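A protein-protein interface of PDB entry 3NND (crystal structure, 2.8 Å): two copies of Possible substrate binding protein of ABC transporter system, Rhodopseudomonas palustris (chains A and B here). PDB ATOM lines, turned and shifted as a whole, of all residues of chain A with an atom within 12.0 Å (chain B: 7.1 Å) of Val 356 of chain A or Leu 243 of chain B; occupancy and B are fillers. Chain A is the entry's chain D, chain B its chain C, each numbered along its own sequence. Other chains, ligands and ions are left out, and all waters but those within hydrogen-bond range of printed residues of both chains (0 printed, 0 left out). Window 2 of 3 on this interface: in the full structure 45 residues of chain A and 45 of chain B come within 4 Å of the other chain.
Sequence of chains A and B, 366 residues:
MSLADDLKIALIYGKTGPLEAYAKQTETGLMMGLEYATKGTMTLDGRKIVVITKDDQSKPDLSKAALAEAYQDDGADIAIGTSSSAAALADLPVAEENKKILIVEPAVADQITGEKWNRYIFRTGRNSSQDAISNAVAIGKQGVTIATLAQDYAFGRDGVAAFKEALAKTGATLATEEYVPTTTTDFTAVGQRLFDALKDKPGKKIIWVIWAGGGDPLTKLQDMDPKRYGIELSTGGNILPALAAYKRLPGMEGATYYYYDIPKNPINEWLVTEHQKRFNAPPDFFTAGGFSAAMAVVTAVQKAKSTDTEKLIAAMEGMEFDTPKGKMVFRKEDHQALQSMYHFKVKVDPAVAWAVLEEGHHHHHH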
ATOM      1  N   LYS A 347     -11.840 -26.158 -25.233  1.00  0.00           N
ATOM      2  CA  LYS A 347     -13.018 -25.378 -24.868  1.00  0.00           C
ATOM      3  C   LYS A 347     -12.617 -24.470 -23.717  1.00  0.00           C
ATOM      4  O   LYS A 347     -12.075 -24.939 -22.728  1.00  0.00           O
ATOM      5  CB  LYS A 347     -14.150 -26.329 -24.480  1.00  0.00           C
ATOM      6  CG  LYS A 347     -15.409 -25.712 -23.918  1.00  0.00           C
ATOM      7  CD  LYS A 347     -16.562 -26.685 -24.169  1.00  0.00           C
ATOM      8  CE  LYS A 347     -17.489 -26.855 -22.968  1.00  0.00           C
ATOM      9  NZ  LYS A 347     -18.393 -28.039 -23.133  1.00  0.00           N
ATOM     10  N   VAL A 348     -12.855 -23.172 -23.853  1.00  0.00           N
ATOM     11  CA  VAL A 348     -12.339 -22.209 -22.884  1.00  0.00           C
ATOM     12  C   VAL A 348     -13.362 -21.674 -21.899  1.00  0.00           C
ATOM     13  O   VAL A 348     -12.983 -21.024 -20.946  1.00  0.00           O
ATOM     14  CB  VAL A 348     -11.718 -20.990 -23.564  1.00  0.00           C
ATOM     15  CG1 VAL A 348     -10.698 -21.426 -24.597  1.00  0.00           C
ATOM     16  CG2 VAL A 348     -12.811 -20.133 -24.187  1.00  0.00           C
ATOM     17  N   ASP A 349     -14.645 -21.925 -22.134  1.00  0.00           N
ATOM     18  CA  ASP A 349     -15.694 -21.379 -21.279  1.00  0.00           C
ATOM     19  C   ASP A 349     -15.454 -21.670 -19.804  1.00  0.00           C
ATOM     20  O   ASP A 349     -15.456 -20.756 -18.983  1.00  0.00           O
ATOM     21  CB  ASP A 349     -17.072 -21.904 -21.696  1.00  0.00           C
ATOM     22  CG  ASP A 349     -17.403 -21.598 -23.152  1.00  0.00           C
ATOM     23  OD1 ASP A 349     -16.564 -21.898 -24.036  1.00  0.00           O
ATOM     24  OD2 ASP A 349     -18.511 -21.069 -23.413  1.00  0.00           O
ATOM     25  N   PRO A 350     -15.252 -22.949 -19.457  1.00  0.00           N
ATOM     26  CA  PRO A 350     -15.023 -23.328 -18.062  1.00  0.00           C
ATOM     27  C   PRO A 350     -13.968 -22.488 -17.345  1.00  0.00           C
ATOM     28  O   PRO A 350     -14.168 -22.164 -16.176  1.00  0.00           O
ATOM     29  CB  PRO A 350     -14.544 -24.773 -18.178  1.00  0.00           C
ATOM     30  CG  PRO A 350     -15.225 -25.279 -19.375  1.00  0.00           C
ATOM     31  CD  PRO A 350     -15.277 -24.127 -20.337  1.00  0.00           C
ATOM     32  N   ALA A 351     -12.873 -22.153 -18.017  1.00  0.00           N
ATOM     33  CA  ALA A 351     -11.731 -21.509 -17.363  1.00  0.00           C
ATOM     34  C   ALA A 351     -11.894 -19.999 -17.264  1.00  0.00           C
ATOM     35  O   ALA A 351     -11.291 -19.343 -16.404  1.00  0.00           O
ATOM     36  CB  ALA A 351     -10.440 -21.861 -18.077  1.00  0.00           C
ATOM     37  N   VAL A 352     -12.708 -19.457 -18.159  1.00  0.00           N
ATOM     38  CA  VAL A 352     -13.040 -18.047 -18.154  1.00  0.00           C
ATOM     39  C   VAL A 352     -14.092 -17.870 -17.091  1.00  0.00           C
ATOM     40  O   VAL A 352     -13.970 -17.023 -16.207  1.00  0.00           O
ATOM     41  CB  VAL A 352     -13.638 -17.613 -19.494  1.00  0.00           C
ATOM     42  CG1 VAL A 352     -14.235 -16.233 -19.379  1.00  0.00           C
ATOM     43  CG2 VAL A 352     -12.589 -17.677 -20.600  1.00  0.00           C
ATOM     44  N   ALA A 353     -15.132 -18.692 -17.184  1.00  0.00           N
ATOM     45  CA  ALA A 353     -16.172 -18.708 -16.176  1.00  0.00           C
ATOM     46  C   ALA A 353     -15.485 -18.823 -14.832  1.00  0.00           C
ATOM     47  O   ALA A 353     -15.889 -18.189 -13.864  1.00  0.00           O
ATOM     48  CB  ALA A 353     -17.121 -19.868 -16.406  1.00  0.00           C
ATOM     49  N   TRP A 354     -14.417 -19.610 -14.789  1.00  0.00           N
ATOM     50  CA  TRP A 354     -13.627 -19.752 -13.577  1.00  0.00           C
ATOM     51  C   TRP A 354     -12.977 -18.420 -13.241  1.00  0.00           C
ATOM     52  O   TRP A 354     -13.336 -17.770 -12.259  1.00  0.00           O
ATOM     53  CB  TRP A 354     -12.576 -20.844 -13.756  1.00  0.00           C
ATOM     54  CG  TRP A 354     -11.765 -21.134 -12.524  1.00  0.00           C
ATOM     55  CD1 TRP A 354     -10.409 -21.325 -12.456  1.00  0.00           C
ATOM     56  CD2 TRP A 354     -12.252 -21.266 -11.187  1.00  0.00           C
ATOM     57  NE1 TRP A 354     -10.028 -21.569 -11.159  1.00  0.00           N
ATOM     58  CE2 TRP A 354     -11.141 -21.538 -10.360  1.00  0.00           C
ATOM     59  CE3 TRP A 354     -13.516 -21.180 -10.605  1.00  0.00           C
ATOM     60  CZ2 TRP A 354     -11.262 -21.729  -8.986  1.00  0.00           C
ATOM     61  CZ3 TRP A 354     -13.632 -21.364  -9.237  1.00  0.00           C
ATOM     62  CH2 TRP A 354     -12.513 -21.637  -8.444  1.00  0.00           C
ATOM     63  N   ALA A 355     -12.045 -18.008 -14.088  1.00  0.00           N
ATOM     64  CA  ALA A 355     -11.307 -16.763 -13.907  1.00  0.00           C
ATOM     65  C   ALA A 355     -12.142 -15.591 -13.385  1.00  0.00           C
ATOM     66  O   ALA A 355     -11.640 -14.762 -12.624  1.00  0.00           O
ATOM     67  CB  ALA A 355     -10.623 -16.376 -15.206  1.00  0.00           C
ATOM     68  N   VAL A 356     -13.400 -15.510 -13.812  1.00  0.00           N
ATOM     69  CA  VAL A 356     -14.250 -14.382 -13.436  1.00  0.00           C
ATOM     70  C   VAL A 356     -14.727 -14.575 -12.009  1.00  0.00           C
ATOM     71  O   VAL A 356     -14.385 -13.794 -11.120  1.00  0.00           O
ATOM     72  CB  VAL A 356     -15.467 -14.170 -14.405  1.00  0.00           C
ATOM     73  CG1 VAL A 356     -15.036 -13.499 -15.715  1.00  0.00           C
ATOM     74  CG2 VAL A 356     -16.193 -15.482 -14.683  1.00  0.00           C
ATOM     75  N   LEU A 357     -15.508 -15.621 -11.781  1.00  0.00           N
ATOM     76  CA  LEU A 357     -15.917 -15.946 -10.423  1.00  0.00           C
ATOM     77  C   LEU A 357     -14.719 -16.415  -9.599  1.00  0.00           C
ATOM     78  O   LEU A 357     -13.788 -15.649  -9.353  1.00  0.00           O
ATOM     79  CB  LEU A 357     -17.038 -16.991 -10.421  1.00  0.00           C
ATOM     80  CG  LEU A 357     -16.866 -18.161  -9.449  1.00  0.00           C
ATOM     81  CD1 LEU A 357     -18.204 -18.735  -8.968  1.00  0.00           C
ATOM     82  CD2 LEU A 357     -16.009 -19.244 -10.098  1.00  0.00           C
ATOM     83  N   ALA B 136      -8.906 -15.795 -23.760  1.00  0.00           N
ATOM     84  CA  ALA B 136     -10.327 -15.815 -23.464  1.00  0.00           C
ATOM     85  C   ALA B 136     -10.609 -15.179 -22.114  1.00  0.00           C
ATOM     86  O   ALA B 136     -11.599 -14.462 -21.949  1.00  0.00           O
ATOM     87  CB  ALA B 136     -10.847 -17.234 -23.506  1.00  0.00           C
ATOM     88  N   VAL B 137      -9.715 -15.431 -21.165  1.00  0.00           N
ATOM     89  CA  VAL B 137      -9.880 -14.982 -19.788  1.00  0.00           C
ATOM     90  C   VAL B 137      -9.709 -13.471 -19.670  1.00  0.00           C
ATOM     91  O   VAL B 137     -10.468 -12.802 -18.968  1.00  0.00           O
ATOM     92  CB  VAL B 137      -8.908 -15.733 -18.844  1.00  0.00           C
ATOM     93  CG1 VAL B 137      -8.658 -14.950 -17.555  1.00  0.00           C
ATOM     94  CG2 VAL B 137      -9.434 -17.145 -18.555  1.00  0.00           C
ATOM     95  N   ILE B 139     -10.348 -11.478 -21.998  1.00  0.00           N
ATOM     96  CA  ILE B 139     -11.473 -10.915 -22.724  1.00  0.00           C
ATOM     97  C   ILE B 139     -12.723 -10.855 -21.862  1.00  0.00           C
ATOM     98  O   ILE B 139     -13.402  -9.827 -21.825  1.00  0.00           O
ATOM     99  CB  ILE B 139     -11.738 -11.673 -24.043  1.00  0.00           C
ATOM    100  CG1 ILE B 139     -10.464 -11.693 -24.890  1.00  0.00           C
ATOM    101  CG2 ILE B 139     -12.882 -11.031 -24.830  1.00  0.00           C
ATOM    102  CD1 ILE B 139     -10.719 -11.675 -26.376  1.00  0.00           C
ATOM    103  N   GLY B 140     -13.013 -11.952 -21.164  1.00  0.00           N
ATOM    104  CA  GLY B 140     -14.160 -12.007 -20.274  1.00  0.00           C
ATOM    105  C   GLY B 140     -14.038 -11.045 -19.102  1.00  0.00           C
ATOM    106  O   GLY B 140     -15.037 -10.565 -18.556  1.00  0.00           O
ATOM    107  N   LYS B 141     -12.800 -10.769 -18.709  1.00  0.00           N
ATOM    108  CA  LYS B 141     -12.533  -9.823 -17.640  1.00  0.00           C
ATOM    109  C   LYS B 141     -12.529  -8.407 -18.178  1.00  0.00           C
ATOM    110  O   LYS B 141     -12.206  -7.480 -17.452  1.00  0.00           O
ATOM    111  CB  LYS B 141     -11.192 -10.119 -16.961  1.00  0.00           C
ATOM    112  CG  LYS B 141     -11.218 -11.332 -16.039  1.00  0.00           C
ATOM    113  CD  LYS B 141     -10.059 -11.315 -15.045  1.00  0.00           C
ATOM    114  CE  LYS B 141      -8.834 -12.068 -15.546  1.00  0.00           C
ATOM    115  NZ  LYS B 141      -8.135 -11.359 -16.664  1.00  0.00           N
ATOM    116  N   GLN B 142     -12.881  -8.237 -19.450  1.00  0.00           N
ATOM    117  CA  GLN B 142     -12.908  -6.902 -20.049  1.00  0.00           C
ATOM    118  C   GLN B 142     -14.311  -6.393 -20.346  1.00  0.00           C
ATOM    119  O   GLN B 142     -15.300  -7.105 -20.191  1.00  0.00           O
ATOM    120  CB  GLN B 142     -12.033  -6.829 -21.301  1.00  0.00           C
ATOM    121  CG  GLN B 142     -10.571  -7.146 -21.029  1.00  0.00           C
ATOM    122  CD  GLN B 142      -9.611  -6.466 -21.995  1.00  0.00           C
ATOM    123  OE1 GLN B 142      -9.438  -5.242 -21.950  1.00  0.00           O
ATOM    124  NE2 GLN B 142      -8.961  -7.257 -22.857  1.00  0.00           N
ATOM    125  N   THR B 170     -26.530  -8.666 -18.936  1.00  0.00           N
ATOM    126  CA  THR B 170     -25.207  -8.987 -19.451  1.00  0.00           C
ATOM    127  C   THR B 170     -24.036  -8.276 -18.767  1.00  0.00           C
ATOM    128  O   THR B 170     -23.089  -8.924 -18.312  1.00  0.00           O
ATOM    129  CB  THR B 170     -25.166  -8.741 -20.965  1.00  0.00           C
ATOM    130  OG1 THR B 170     -25.479  -9.960 -21.650  1.00  0.00           O
ATOM    131  CG2 THR B 170     -23.799  -8.258 -21.395  1.00  0.00           C
ATOM    132  N   LEU B 240     -17.997 -12.490 -28.627  1.00  0.00           N
ATOM    133  CA  LEU B 240     -18.366 -12.254 -27.237  1.00  0.00           C
ATOM    134  C   LEU B 240     -17.497 -13.060 -26.296  1.00  0.00           C
ATOM    135  O   LEU B 240     -17.038 -14.148 -26.643  1.00  0.00           O
ATOM    136  CB  LEU B 240     -19.837 -12.600 -27.007  1.00  0.00           C
ATOM    137  CG  LEU B 240     -20.795 -11.513 -27.493  1.00  0.00           C
ATOM    138  CD1 LEU B 240     -22.241 -11.972 -27.494  1.00  0.00           C
ATOM    139  CD2 LEU B 240     -20.626 -10.294 -26.631  1.00  0.00           C
ATOM    140  N   PRO B 241     -17.241 -12.518 -25.100  1.00  0.00           N
ATOM    141  CA  PRO B 241     -16.525 -13.297 -24.091  1.00  0.00           C
ATOM    142  C   PRO B 241     -17.246 -14.611 -23.791  1.00  0.00           C
ATOM    143  O   PRO B 241     -18.471 -14.637 -23.740  1.00  0.00           O
ATOM    144  CB  PRO B 241     -16.562 -12.381 -22.866  1.00  0.00           C
ATOM    145  CG  PRO B 241     -16.593 -11.002 -23.447  1.00  0.00           C
ATOM    146  CD  PRO B 241     -17.449 -11.122 -24.677  1.00  0.00           C
ATOM    147  N   ALA B 242     -16.482 -15.686 -23.617  1.00  0.00           N
ATOM    148  CA  ALA B 242     -17.035 -16.983 -23.219  1.00  0.00           C
ATOM    149  C   ALA B 242     -17.569 -16.934 -21.787  1.00  0.00           C
ATOM    150  O   ALA B 242     -16.915 -17.376 -20.843  1.00  0.00           O
ATOM    151  CB  ALA B 242     -15.988 -18.083 -23.370  1.00  0.00           C
ATOM    152  N   LEU B 243     -18.761 -16.372 -21.635  1.00  0.00           N
ATOM    153  CA  LEU B 243     -19.405 -16.273 -20.336  1.00  0.00           C
ATOM    154  C   LEU B 243     -20.851 -16.660 -20.516  1.00  0.00           C
ATOM    155  O   LEU B 243     -21.500 -16.213 -21.460  1.00  0.00           O
ATOM    156  CB  LEU B 243     -19.298 -14.849 -19.785  1.00  0.00           C
ATOM    157  CG  LEU B 243     -17.918 -14.441 -19.253  1.00  0.00           C
ATOM    158  CD1 LEU B 243     -17.876 -12.947 -18.981  1.00  0.00           C
ATOM    159  CD2 LEU B 243     -17.545 -15.231 -18.006  1.00  0.00           C
ATOM    160  N   ALA B 244     -21.350 -17.508 -19.625  1.00  0.00           N
ATOM    161  CA  ALA B 244     -22.711 -18.003 -19.741  1.00  0.00           C
ATOM    162  C   ALA B 244     -23.674 -16.864 -20.050  1.00  0.00           C
ATOM    163  O   ALA B 244     -24.619 -17.036 -20.825  1.00  0.00           O
ATOM    164  CB  ALA B 244     -23.125 -18.730 -18.480  1.00  0.00           C
ATOM    165  N   ALA B 245     -23.415 -15.698 -19.461  1.00  0.00           N
ATOM    166  CA  ALA B 245     -24.270 -14.517 -19.652  1.00  0.00           C
ATOM    167  C   ALA B 245     -24.555 -14.197 -21.125  1.00  0.00           C
ATOM    168  O   ALA B 245     -25.664 -13.795 -21.463  1.00  0.00           O
ATOM    169  CB  ALA B 245     -23.687 -13.296 -18.929  1.00  0.00           C
ATOM    170  N   TYR B 246     -23.552 -14.376 -21.986  1.00  0.00           N
ATOM    171  CA  TYR B 246     -23.731 -14.265 -23.434  1.00  0.00           C
ATOM    172  C   TYR B 246     -23.985 -15.650 -24.012  1.00  0.00           C
ATOM    173  O   TYR B 246     -25.055 -15.925 -24.552  1.00  0.00           O
ATOM    174  CB  TYR B 246     -22.495 -13.652 -24.108  1.00  0.00           C
ATOM    175  CG  TYR B 246     -21.951 -12.390 -23.449  1.00  0.00           C
ATOM    176  CD1 TYR B 246     -22.488 -11.139 -23.731  1.00  0.00           C
ATOM    177  CD2 TYR B 246     -20.884 -12.452 -22.566  1.00  0.00           C
ATOM    178  CE1 TYR B 246     -21.988  -9.990 -23.142  1.00  0.00           C
ATOM    179  CE2 TYR B 246     -20.376 -11.307 -21.966  1.00  0.00           C
ATOM    180  CZ  TYR B 246     -20.932 -10.079 -22.254  1.00  0.00           C
ATOM    181  OH  TYR B 246     -20.422  -8.942 -21.651  1.00  0.00           O
ATOM    182  N   THR B 256     -17.188 -21.671 -26.918  1.00  0.00           N
ATOM    183  CA  THR B 256     -16.056 -21.046 -27.587  1.00  0.00           C
ATOM    184  C   THR B 256     -14.884 -22.022 -27.621  1.00  0.00           C
ATOM    185  O   THR B 256     -14.404 -22.453 -26.575  1.00  0.00           O
ATOM    186  CB  THR B 256     -15.616 -19.762 -26.850  1.00  0.00           C
ATOM    187  OG1 THR B 256     -16.721 -18.857 -26.749  1.00  0.00           O
ATOM    188  CG2 THR B 256     -14.461 -19.090 -27.583  1.00  0.00           C
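CA of Lys 347 of chain A touches O of Thr 256 of chain B, 3.7 Å away. CG2 of Val 348 of chain A touches CB of Ala 136 of chain B, at 3.6 Å. Val 348 of chain A touches Ala 242 of chain B. Ala 242 of chain B touches Asp 349 of chain A. Val 137 of chain B touches Ala 351 of chain A (CG2 to O, 3.6 Å). CG2 of Val 352 of chain A touches CB of Ala 136 of chain B, at 3.4 Å. Val 137 of chain B touches Val 352 of chain A. O of Ala 242 of chain B touches CG1 of Val 352 of chain A (3.3 Å). Val 137 of chain B touches Ala 355 of chain A (CG1 to CB, 3.4 Å). Val 356 of chain A touches Leu 243 of chain B.
Of the 11 printed residues of chain A, 7 touch a printed residue of chain B. Hydrophobic or aromatic side chains of chain A that line the printed part of chain B: Val 348, Val 352, Ala 355 and Val 356. Of the 15 printed residues of chain B, 5 touch a printed residue of chain A. Printed residues of chain B that touch a printed residue of chain A: Ala 136, Val 137, Ala 242, Leu 243 and Thr 256. Hydrophobic or aromatic side chains of chain B within 4 Å of the printed part of chain A: Ala 136, Val 137, Ala 242 and Leu 243. Among the printed residues, no Asp or Glu carboxylate lies within 4 Å of a Lys or Arg side-chain nitrogen of the other chain.
N of Val 348 of chain A is in hydrogen-bond range of O of Thr 256 of chain B, 3.2 Å away. The side-chain carboxylate of Asp 349 of chain A sits at hydrogen-bond distance from the backbone NH of Thr 256 of chain B.
Printed residues of chain B within 4 Å of Val 352 of chain A: Ala 136 (3.4 Å), Val 137 (3.7 Å), Ala 242 (3.3 Å) and Leu 243 (3.7 Å). Printed residues of chain B within 4 Å of Ala 355 of chain A: Val 137 (3.4 Å). Of the printed residues of chain B, Val 356 of chain A touches Leu 243. Leu 357 of chain A touches none of the printed residues of chain B. Val 137 of chain B touches just these residues of chain A: Ala 351, Val 352 and Ala 355. Ile 139 of chain B touches none of the printed residues of chain A. No residue of chain A comes within 4 Å of Lys 141 of chain B. Ala 244 of chain B touches none of the printed residues of chain A. Ala 245 of chain B touches none of the printed residues of chain A. The nearest residue of chain B that does not touch Val 356 of chain A is Gly 140 of chain B (4.1 Å). The nearest residue of chain A that does not touch Leu 243 of chain B is Ala 353 of chain A (4.2 Å). The nearest printed residue of chain B that does not touch Val 348 of chain A is Val 137 of chain B (5.8 Å).
No position is printed for both chains.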
